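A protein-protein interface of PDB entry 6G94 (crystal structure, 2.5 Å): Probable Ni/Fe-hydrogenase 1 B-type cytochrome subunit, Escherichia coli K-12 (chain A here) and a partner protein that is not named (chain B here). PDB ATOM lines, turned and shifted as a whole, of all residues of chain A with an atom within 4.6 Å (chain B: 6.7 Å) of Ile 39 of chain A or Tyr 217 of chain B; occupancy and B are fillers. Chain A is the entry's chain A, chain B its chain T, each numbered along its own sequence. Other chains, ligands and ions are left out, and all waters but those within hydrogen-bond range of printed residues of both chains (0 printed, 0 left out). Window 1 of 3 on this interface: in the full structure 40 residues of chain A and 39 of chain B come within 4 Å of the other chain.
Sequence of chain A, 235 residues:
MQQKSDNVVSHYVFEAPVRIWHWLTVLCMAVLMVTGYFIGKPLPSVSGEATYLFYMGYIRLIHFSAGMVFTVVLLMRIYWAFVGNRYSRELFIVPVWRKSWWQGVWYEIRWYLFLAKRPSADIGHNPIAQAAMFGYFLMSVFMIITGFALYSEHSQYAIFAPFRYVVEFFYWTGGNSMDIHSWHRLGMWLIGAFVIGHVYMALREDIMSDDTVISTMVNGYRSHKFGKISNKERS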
ATOM      1  N   THR A  35      -4.031 -18.547  33.562  1.00  0.00           N
ATOM      2  CA  THR A  35      -4.395 -17.215  33.025  1.00  0.00           C
ATOM      3  C   THR A  35      -3.587 -16.120  33.686  1.00  0.00           C
ATOM      4  O   THR A  35      -3.008 -15.277  32.994  1.00  0.00           O
ATOM      5  CB  THR A  35      -5.907 -16.831  33.127  1.00  0.00           C
ATOM      6  OG1 THR A  35      -6.339 -16.835  34.491  1.00  0.00           O
ATOM      7  CG2 THR A  35      -6.759 -17.757  32.315  1.00  0.00           C
ATOM      8  N   GLY A  36      -3.550 -16.126  35.017  1.00  0.00           N
ATOM      9  CA  GLY A  36      -2.814 -15.112  35.765  1.00  0.00           C
ATOM     10  C   GLY A  36      -1.326 -15.071  35.418  1.00  0.00           C
ATOM     11  O   GLY A  36      -0.694 -14.001  35.409  1.00  0.00           O
ATOM     12  N   TYR A  37      -0.767 -16.250  35.131  1.00  0.00           N
ATOM     13  CA  TYR A  37       0.597 -16.351  34.642  1.00  0.00           C
ATOM     14  C   TYR A  37       0.808 -15.462  33.409  1.00  0.00           C
ATOM     15  O   TYR A  37       1.749 -14.687  33.366  1.00  0.00           O
ATOM     16  CB  TYR A  37       0.959 -17.808  34.318  1.00  0.00           C
ATOM     17  CG  TYR A  37       2.388 -17.953  33.854  1.00  0.00           C
ATOM     18  CD1 TYR A  37       3.444 -17.780  34.752  1.00  0.00           C
ATOM     19  CD2 TYR A  37       2.691 -18.226  32.514  1.00  0.00           C
ATOM     20  CE1 TYR A  37       4.759 -17.884  34.339  1.00  0.00           C
ATOM     21  CE2 TYR A  37       4.008 -18.330  32.091  1.00  0.00           C
ATOM     22  CZ  TYR A  37       5.036 -18.159  33.010  1.00  0.00           C
ATOM     23  OH  TYR A  37       6.347 -18.253  32.624  1.00  0.00           O
ATOM     24  N   PHE A  38      -0.085 -15.590  32.427  1.00  0.00           N
ATOM     25  CA  PHE A  38       0.014 -14.875  31.165  1.00  0.00           C
ATOM     26  C   PHE A  38      -0.477 -13.417  31.200  1.00  0.00           C
ATOM     27  O   PHE A  38      -0.276 -12.675  30.239  1.00  0.00           O
ATOM     28  CB  PHE A  38      -0.701 -15.664  30.078  1.00  0.00           C
ATOM     29  CG  PHE A  38      -0.012 -16.931  29.722  1.00  0.00           C
ATOM     30  CD1 PHE A  38       1.335 -16.934  29.413  1.00  0.00           C
ATOM     31  CD2 PHE A  38      -0.709 -18.134  29.698  1.00  0.00           C
ATOM     32  CE1 PHE A  38       1.982 -18.118  29.091  1.00  0.00           C
ATOM     33  CE2 PHE A  38      -0.072 -19.326  29.376  1.00  0.00           C
ATOM     34  CZ  PHE A  38       1.283 -19.317  29.078  1.00  0.00           C
ATOM     35  N   ILE A  39      -1.100 -13.002  32.299  1.00  0.00           N
ATOM     36  CA  ILE A  39      -1.374 -11.587  32.505  1.00  0.00           C
ATOM     37  C   ILE A  39      -0.070 -10.865  32.822  1.00  0.00           C
ATOM     38  O   ILE A  39       0.102  -9.711  32.471  1.00  0.00           O
ATOM     39  CB  ILE A  39      -2.444 -11.364  33.600  1.00  0.00           C
ATOM     40  CG1 ILE A  39      -3.824 -11.828  33.081  1.00  0.00           C
ATOM     41  CG2 ILE A  39      -2.506  -9.909  34.064  1.00  0.00           C
ATOM     42  CD1 ILE A  39      -4.891 -12.030  34.140  1.00  0.00           C
ATOM     43  N   GLY A  40       0.869 -11.566  33.443  1.00  0.00           N
ATOM     44  CA  GLY A  40       2.131 -10.973  33.857  1.00  0.00           C
ATOM     45  C   GLY A  40       3.252 -11.241  32.861  1.00  0.00           C
ATOM     46  O   GLY A  40       4.053 -10.349  32.562  1.00  0.00           O
ATOM     47  N   LYS A  41       3.325 -12.472  32.357  1.00  0.00           N
ATOM     48  CA  LYS A  41       4.239 -12.808  31.269  1.00  0.00           C
ATOM     49  C   LYS A  41       3.403 -13.213  30.054  1.00  0.00           C
ATOM     50  O   LYS A  41       3.164 -14.416  29.826  1.00  0.00           O
ATOM     51  CB  LYS A  41       5.207 -13.920  31.684  1.00  0.00           C
ATOM     52  CG  LYS A  41       6.212 -13.506  32.744  1.00  0.00           C
ATOM     53  CD  LYS A  41       7.405 -12.771  32.130  1.00  0.00           C
ATOM     54  CE  LYS A  41       8.357 -12.229  33.202  1.00  0.00           C
ATOM     55  NZ  LYS A  41       9.396 -11.306  32.649  1.00  0.00           N
ATOM     56  N   PRO A  42       2.922 -12.212  29.286  1.00  0.00           N
ATOM     57  CA  PRO A  42       1.970 -12.454  28.183  1.00  0.00           C
ATOM     58  C   PRO A  42       2.542 -13.313  27.081  1.00  0.00           C
ATOM     59  O   PRO A  42       3.764 -13.380  26.911  1.00  0.00           O
ATOM     60  CB  PRO A  42       1.693 -11.059  27.645  1.00  0.00           C
ATOM     61  CG  PRO A  42       1.972 -10.160  28.808  1.00  0.00           C
ATOM     62  CD  PRO A  42       3.158 -10.771  29.486  1.00  0.00           C
ATOM     63  N   ILE A  59      -8.323 -13.565  28.184  1.00  0.00           N
ATOM     64  CA  ILE A  59      -7.561 -14.138  29.277  1.00  0.00           C
ATOM     65  C   ILE A  59      -7.897 -13.429  30.585  1.00  0.00           C
ATOM     66  O   ILE A  59      -8.041 -14.054  31.612  1.00  0.00           O
ATOM     67  CB  ILE A  59      -6.060 -14.033  28.965  1.00  0.00           C
ATOM     68  CG1 ILE A  59      -5.686 -15.031  27.890  1.00  0.00           C
ATOM     69  CG2 ILE A  59      -5.176 -14.195  30.197  1.00  0.00           C
ATOM     70  CD1 ILE A  59      -4.328 -14.723  27.297  1.00  0.00           C
ATOM     71  N   ARG A  60      -8.011 -12.116  30.526  1.00  0.00           N
ATOM     72  CA  ARG A  60      -8.298 -11.321  31.710  1.00  0.00           C
ATOM     73  C   ARG A  60      -9.724 -11.563  32.161  1.00  0.00           C
ATOM     74  O   ARG A  60     -10.023 -11.528  33.333  1.00  0.00           O
ATOM     75  CB  ARG A  60      -8.034  -9.831  31.442  1.00  0.00           C
ATOM     76  CG  ARG A  60      -6.625  -9.519  30.953  1.00  0.00           C
ATOM     77  CD  ARG A  60      -6.317  -8.035  30.775  1.00  0.00           C
ATOM     78  NE  ARG A  60      -6.915  -7.205  31.814  1.00  0.00           N
ATOM     79  CZ  ARG A  60      -7.874  -6.334  31.582  1.00  0.00           C
ATOM     80  NH1 ARG A  60      -8.406  -5.637  32.558  1.00  0.00           N
ATOM     81  NH2 ARG A  60      -8.301  -6.184  30.355  1.00  0.00           N
ATOM     82  N   HIS A  63     -10.052 -14.911  33.699  1.00  0.00           N
ATOM     83  CA  HIS A  63      -9.438 -14.776  35.009  1.00  0.00           C
ATOM     84  C   HIS A  63     -10.383 -14.161  36.034  1.00  0.00           C
ATOM     85  O   HIS A  63     -10.617 -14.731  37.086  1.00  0.00           O
ATOM     86  CB  HIS A  63      -8.142 -13.979  34.913  1.00  0.00           C
ATOM     87  CG  HIS A  63      -7.291 -14.054  36.146  1.00  0.00           C
ATOM     88  ND1 HIS A  63      -6.418 -15.091  36.385  1.00  0.00           N
ATOM     89  CD2 HIS A  63      -7.173 -13.215  37.207  1.00  0.00           C
ATOM     90  CE1 HIS A  63      -5.810 -14.893  37.542  1.00  0.00           C
ATOM     91  NE2 HIS A  63      -6.249 -13.765  38.062  1.00  0.00           N
ATOM     92  N   HIS B 187      -3.383   3.667  32.139  1.00  0.00           N
ATOM     93  CA  HIS B 187      -3.882   2.502  31.443  1.00  0.00           C
ATOM     94  C   HIS B 187      -5.403   2.585  31.209  1.00  0.00           C
ATOM     95  O   HIS B 187      -5.931   1.962  30.284  1.00  0.00           O
ATOM     96  CB  HIS B 187      -3.527   1.283  32.284  1.00  0.00           C
ATOM     97  CG  HIS B 187      -3.733  -0.032  31.608  1.00  0.00           C
ATOM     98  ND1 HIS B 187      -3.022  -0.415  30.489  1.00  0.00           N
ATOM     99  CD2 HIS B 187      -4.530  -1.079  31.932  1.00  0.00           C
ATOM    100  CE1 HIS B 187      -3.389  -1.636  30.143  1.00  0.00           C
ATOM    101  NE2 HIS B 187      -4.308  -2.058  30.996  1.00  0.00           N
ATOM    102  N   PHE B 196      -3.373  -3.630  23.624  1.00  0.00           N
ATOM    103  CA  PHE B 196      -3.211  -4.359  24.878  1.00  0.00           C
ATOM    104  C   PHE B 196      -4.191  -5.505  24.976  1.00  0.00           C
ATOM    105  O   PHE B 196      -3.786  -6.638  25.137  1.00  0.00           O
ATOM    106  CB  PHE B 196      -3.368  -3.423  26.077  1.00  0.00           C
ATOM    107  CG  PHE B 196      -3.377  -4.131  27.406  1.00  0.00           C
ATOM    108  CD1 PHE B 196      -2.184  -4.483  28.027  1.00  0.00           C
ATOM    109  CD2 PHE B 196      -4.570  -4.412  28.056  1.00  0.00           C
ATOM    110  CE1 PHE B 196      -2.178  -5.115  29.260  1.00  0.00           C
ATOM    111  CE2 PHE B 196      -4.568  -5.040  29.292  1.00  0.00           C
ATOM    112  CZ  PHE B 196      -3.371  -5.391  29.896  1.00  0.00           C
ATOM    113  N   PHE B 201       1.645  -6.560  21.062  1.00  0.00           N
ATOM    114  CA  PHE B 201       2.680  -5.942  21.878  1.00  0.00           C
ATOM    115  C   PHE B 201       3.993  -5.714  21.138  1.00  0.00           C
ATOM    116  O   PHE B 201       4.394  -6.493  20.271  1.00  0.00           O
ATOM    117  CB  PHE B 201       2.965  -6.813  23.099  1.00  0.00           C
ATOM    118  CG  PHE B 201       1.771  -7.063  23.974  1.00  0.00           C
ATOM    119  CD1 PHE B 201       1.231  -6.039  24.749  1.00  0.00           C
ATOM    120  CD2 PHE B 201       1.208  -8.334  24.053  1.00  0.00           C
ATOM    121  CE1 PHE B 201       0.136  -6.276  25.572  1.00  0.00           C
ATOM    122  CE2 PHE B 201       0.128  -8.574  24.875  1.00  0.00           C
ATOM    123  CZ  PHE B 201      -0.413  -7.544  25.632  1.00  0.00           C
ATOM    124  N   VAL B 202       4.668  -4.634  21.499  1.00  0.00           N
ATOM    125  CA  VAL B 202       6.043  -4.419  21.073  1.00  0.00           C
ATOM    126  C   VAL B 202       6.867  -5.413  21.871  1.00  0.00           C
ATOM    127  O   VAL B 202       6.696  -5.509  23.096  1.00  0.00           O
ATOM    128  CB  VAL B 202       6.535  -2.984  21.386  1.00  0.00           C
ATOM    129  CG1 VAL B 202       8.002  -2.827  21.015  1.00  0.00           C
ATOM    130  CG2 VAL B 202       5.710  -1.938  20.668  1.00  0.00           C
ATOM    131  N   TYR B 214       1.888  -0.338  18.657  1.00  0.00           N
ATOM    132  CA  TYR B 214       1.346  -1.380  19.522  1.00  0.00           C
ATOM    133  C   TYR B 214       1.670  -1.115  20.976  1.00  0.00           C
ATOM    134  O   TYR B 214       2.514  -0.276  21.283  1.00  0.00           O
ATOM    135  CB  TYR B 214       1.864  -2.762  19.126  1.00  0.00           C
ATOM    136  CG  TYR B 214       1.187  -3.340  17.919  1.00  0.00           C
ATOM    137  CD1 TYR B 214       0.317  -2.571  17.147  1.00  0.00           C
ATOM    138  CD2 TYR B 214       1.434  -4.646  17.523  1.00  0.00           C
ATOM    139  CE1 TYR B 214      -0.305  -3.097  16.018  1.00  0.00           C
ATOM    140  CE2 TYR B 214       0.829  -5.184  16.389  1.00  0.00           C
ATOM    141  CZ  TYR B 214      -0.042  -4.410  15.637  1.00  0.00           C
ATOM    142  OH  TYR B 214      -0.654  -4.942  14.512  1.00  0.00           O
ATOM    143  N   CYS B 215       0.974  -1.834  21.860  1.00  0.00           N
ATOM    144  CA  CYS B 215       1.099  -1.689  23.314  1.00  0.00           C
ATOM    145  C   CYS B 215       2.525  -1.992  23.854  1.00  0.00           C
ATOM    146  O   CYS B 215       3.243  -2.862  23.334  1.00  0.00           O
ATOM    147  CB  CYS B 215       0.070  -2.579  23.981  1.00  0.00           C
ATOM    148  SG  CYS B 215       0.130  -2.528  25.753  1.00  0.00           S
ATOM    149  N   LEU B 216       2.914  -1.265  24.899  1.00  0.00           N
ATOM    150  CA  LEU B 216       4.278  -1.337  25.439  1.00  0.00           C
ATOM    151  C   LEU B 216       4.334  -2.066  26.778  1.00  0.00           C
ATOM    152  O   LEU B 216       5.263  -1.874  27.582  1.00  0.00           O
ATOM    153  CB  LEU B 216       4.871   0.069  25.593  1.00  0.00           C
ATOM    154  CG  LEU B 216       4.917   0.937  24.328  1.00  0.00           C
ATOM    155  CD1 LEU B 216       5.183   2.378  24.716  1.00  0.00           C
ATOM    156  CD2 LEU B 216       5.951   0.459  23.320  1.00  0.00           C
ATOM    157  N   TYR B 217       3.337  -2.912  27.006  1.00  0.00           N
ATOM    158  CA  TYR B 217       3.179  -3.630  28.264  1.00  0.00           C
ATOM    159  C   TYR B 217       4.372  -4.575  28.494  1.00  0.00           C
ATOM    160  O   TYR B 217       4.915  -4.614  29.591  1.00  0.00           O
ATOM    161  CB  TYR B 217       1.834  -4.368  28.230  1.00  0.00           C
ATOM    162  CG  TYR B 217       1.390  -5.143  29.456  1.00  0.00           C
ATOM    163  CD1 TYR B 217       1.137  -4.500  30.660  1.00  0.00           C
ATOM    164  CD2 TYR B 217       1.115  -6.499  29.376  1.00  0.00           C
ATOM    165  CE1 TYR B 217       0.671  -5.187  31.771  1.00  0.00           C
ATOM    166  CE2 TYR B 217       0.643  -7.194  30.481  1.00  0.00           C
ATOM    167  CZ  TYR B 217       0.424  -6.527  31.678  1.00  0.00           C
ATOM    168  OH  TYR B 217      -0.041  -7.188  32.787  1.00  0.00           O
ATOM    169  N   LYS B 218       4.789  -5.295  27.442  1.00  0.00           N
ATOM    170  CA  LYS B 218       5.895  -6.260  27.504  1.00  0.00           C
ATOM    171  C   LYS B 218       7.238  -5.566  27.445  1.00  0.00           C
ATOM    172  O   LYS B 218       8.289  -6.231  27.513  1.00  0.00           O
ATOM    173  CB  LYS B 218       5.864  -7.227  26.331  1.00  0.00           C
ATOM    174  CG  LYS B 218       4.722  -8.221  26.286  1.00  0.00           C
ATOM    175  CD  LYS B 218       4.972  -9.119  25.089  1.00  0.00           C
ATOM    176  CE  LYS B 218       4.780 -10.573  25.414  1.00  0.00           C
ATOM    177  NZ  LYS B 218       5.165 -11.312  24.184  1.00  0.00           N
ATOM    178  N   MET B 219       7.216  -4.247  27.252  1.00  0.00           N
ATOM    179  CA  MET B 219       8.446  -3.472  27.337  1.00  0.00           C
ATOM    180  C   MET B 219       8.544  -2.841  28.726  1.00  0.00           C
ATOM    181  O   MET B 219       9.450  -2.073  29.015  1.00  0.00           O
ATOM    182  CB  MET B 219       8.526  -2.436  26.214  1.00  0.00           C
ATOM    183  CG  MET B 219       8.431  -3.023  24.808  1.00  0.00           C
ATOM    184  SD  MET B 219       9.626  -4.348  24.505  1.00  0.00           S
ATOM    185  CE  MET B 219      11.185  -3.503  24.663  1.00  0.00           C
ATOM    186  N   GLY B 220       7.594  -3.188  29.589  1.00  0.00           N
ATOM    187  CA  GLY B 220       7.653  -2.819  30.990  1.00  0.00           C
ATOM    188  C   GLY B 220       6.730  -1.697  31.408  1.00  0.00           C
ATOM    189  O   GLY B 220       6.832  -1.228  32.543  1.00  0.00           O
ATOM    190  N   CYS B 221       5.830  -1.267  30.520  1.00  0.00           N
ATOM    191  CA  CYS B 221       4.985  -0.117  30.815  1.00  0.00           C
ATOM    192  C   CYS B 221       4.265  -0.290  32.141  1.00  0.00           C
ATOM    193  O   CYS B 221       3.648  -1.315  32.386  1.00  0.00           O
ATOM    194  CB  CYS B 221       3.972   0.128  29.696  1.00  0.00           C
ATOM    195  SG  CYS B 221       2.815   1.503  30.023  1.00  0.00           S
ATOM    196  N   LYS B 222       4.376   0.708  33.004  1.00  0.00           N
ATOM    197  CA  LYS B 222       3.755   0.654  34.321  1.00  0.00           C
ATOM    198  C   LYS B 222       2.472   1.476  34.356  1.00  0.00           C
ATOM    199  O   LYS B 222       1.941   1.805  35.434  1.00  0.00           O
ATOM    200  CB  LYS B 222       4.727   1.102  35.415  1.00  0.00           C
ATOM    201  CG  LYS B 222       5.989   0.264  35.501  1.00  0.00           C
ATOM    202  CD  LYS B 222       5.652  -1.217  35.586  1.00  0.00           C
ATOM    203  CE  LYS B 222       6.874  -2.077  35.863  1.00  0.00           C
ATOM    204  NZ  LYS B 222       7.990  -1.869  34.905  1.00  0.00           N
ATOM    205  N   PRO B 224      -0.520   0.507  33.856  1.00  0.00           N
ATOM    206  CA  PRO B 224      -1.593  -0.164  34.619  1.00  0.00           C
ATOM    207  C   PRO B 224      -1.665   0.135  36.116  1.00  0.00           C
ATOM    208  O   PRO B 224      -2.693  -0.108  36.739  1.00  0.00           O
ATOM    209  CB  PRO B 224      -1.303  -1.641  34.383  1.00  0.00           C
ATOM    210  CG  PRO B 224      -0.698  -1.665  33.021  1.00  0.00           C
ATOM    211  CD  PRO B 224       0.120  -0.423  32.900  1.00  0.00           C
ATOM    212  N   GLY B 248       7.490   2.978  27.433  1.00  0.00           N
ATOM    213  CA  GLY B 248       6.483   2.663  28.442  1.00  0.00           C
ATOM    214  C   GLY B 248       6.521   3.629  29.606  1.00  0.00           C
ATOM    215  O   GLY B 248       7.543   4.247  29.874  1.00  0.00           O
ATOM    216  N   TYR B 264      11.910  -2.069  32.463  1.00  0.00           N
ATOM    217  CA  TYR B 264      11.639  -2.867  31.279  1.00  0.00           C
ATOM    218  C   TYR B 264      11.098  -4.271  31.529  1.00  0.00           C
ATOM    219  O   TYR B 264      11.032  -5.088  30.598  1.00  0.00           O
ATOM    220  CB  TYR B 264      12.884  -2.924  30.404  1.00  0.00           C
ATOM    221  CG  TYR B 264      13.338  -1.547  30.015  1.00  0.00           C
ATOM    222  CD1 TYR B 264      12.598  -0.763  29.104  1.00  0.00           C
ATOM    223  CD2 TYR B 264      14.484  -0.997  30.582  1.00  0.00           C
ATOM    224  CE1 TYR B 264      13.007   0.528  28.766  1.00  0.00           C
ATOM    225  CE2 TYR B 264      14.902   0.282  30.245  1.00  0.00           C
ATOM    226  CZ  TYR B 264      14.164   1.049  29.336  1.00  0.00           C
ATOM    227  OH  TYR B 264      14.582   2.331  28.999  1.00  0.00           O
ATOM    228  N   SER B 265      10.702  -4.545  32.771  1.00  0.00           N
ATOM    229  CA  SER B 265      10.173  -5.857  33.121  1.00  0.00           C
ATOM    230  C   SER B 265       8.761  -5.780  33.722  1.00  0.00           C
ATOM    231  O   SER B 265       8.432  -4.825  34.457  1.00  0.00           O
ATOM    232  CB  SER B 265      11.130  -6.603  34.061  1.00  0.00           C
ATOM    233  OG  SER B 265      11.573  -5.757  35.115  1.00  0.00           O
ATOM    234  N   ARG B 266       7.935  -6.780  33.392  1.00  0.00           N
ATOM    235  CA  ARG B 266       6.587  -6.881  33.961  1.00  0.00           C
ATOM    236  C   ARG B 266       6.618  -7.286  35.419  1.00  0.00           C
ATOM    237  O   ARG B 266       5.843  -6.773  36.222  1.00  0.00           O
ATOM    238  CB  ARG B 266       5.715  -7.851  33.176  1.00  0.00           C
ATOM    239  CG  ARG B 266       5.260  -7.285  31.843  1.00  0.00           C
ATOM    240  CD  ARG B 266       3.812  -6.840  31.916  1.00  0.00           C
ATOM    241  NE  ARG B 266       3.536  -5.931  33.030  1.00  0.00           N
ATOM    242  CZ  ARG B 266       3.762  -4.613  33.015  1.00  0.00           C
ATOM    243  NH1 ARG B 266       4.267  -4.009  31.930  1.00  0.00           N
ATOM    244  NH2 ARG B 266       3.470  -3.892  34.094  1.00  0.00           N
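OH of Tyr 217 of chain B lies within hydrogen-bond range of O of Ile 39 of chain A (2.5 Å).
Printed residues of chain A that touch a printed residue of chain B: Ile 39, Gly 40, Pro 42 and Arg 60.
Hydrophobic or aromatic side chains of chain A that line the printed part of chain B: Ile 39 and Pro 42.
Hydrophobic or aromatic side chains of chain B that line the printed part of chain A: Phe 196 and Tyr 217.
Among the printed residues, 5 pairs touch across the chains.
Among the printed residues, no Asp or Glu carboxylate lies within 4 Å of a Lys or Arg side-chain nitrogen of the other chain.
Of chain B, only Tyr 217 (2.5 Å) comes within 4 Å of Ile 39 of chain A.
Of chain A, only Ile 39 (2.5 Å) and Pro 42 (3.7 Å) come within 4 Å of Tyr 217 of chain B.
Of the printed residues of chain B, Arg 60 of chain A touches Phe 196 (3.8 Å).
Of the printed residues of chain A, Phe 196 of chain B touches Arg 60.
Printed residues of chain A within 4 Å of Lys 218 of chain B: Pro 42.
Of the printed residues of chain B, Gly 40 of chain A touches Arg 266 (3.1 Å).
Of the printed residues of chain B, Pro 42 of chain A touches Tyr 217 (3.7 Å) and Lys 218 (3.3 Å).
Lys 41 of chain A touches none of the printed residues of chain B.
The nearest printed residue of chain B that does not touch Gly 40 of chain A is Tyr 217 of chain B (4.5 Å).
SG of Cys 215 of chain B lies close to N of Tyr 217 of chain B (3.5 Å).
NH1 of Arg 266 of chain B sits at hydrogen-bond distance from O of Cys 221 of chain B, 2.8 Å away.
NH1 of Arg 266 of chain B lies within hydrogen-bond range of O of Tyr 217 of chain B (2.5 Å).
Among the printed residues, pairs that only touch across the chains: Gly 40 of chain A with Arg 266 of chain B, Pro 42 of chain A with Tyr 217 of chain B, Pro 42 of chain A with Lys 218 of chain B and Arg 60 of chain A with Phe 196 of chain B.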
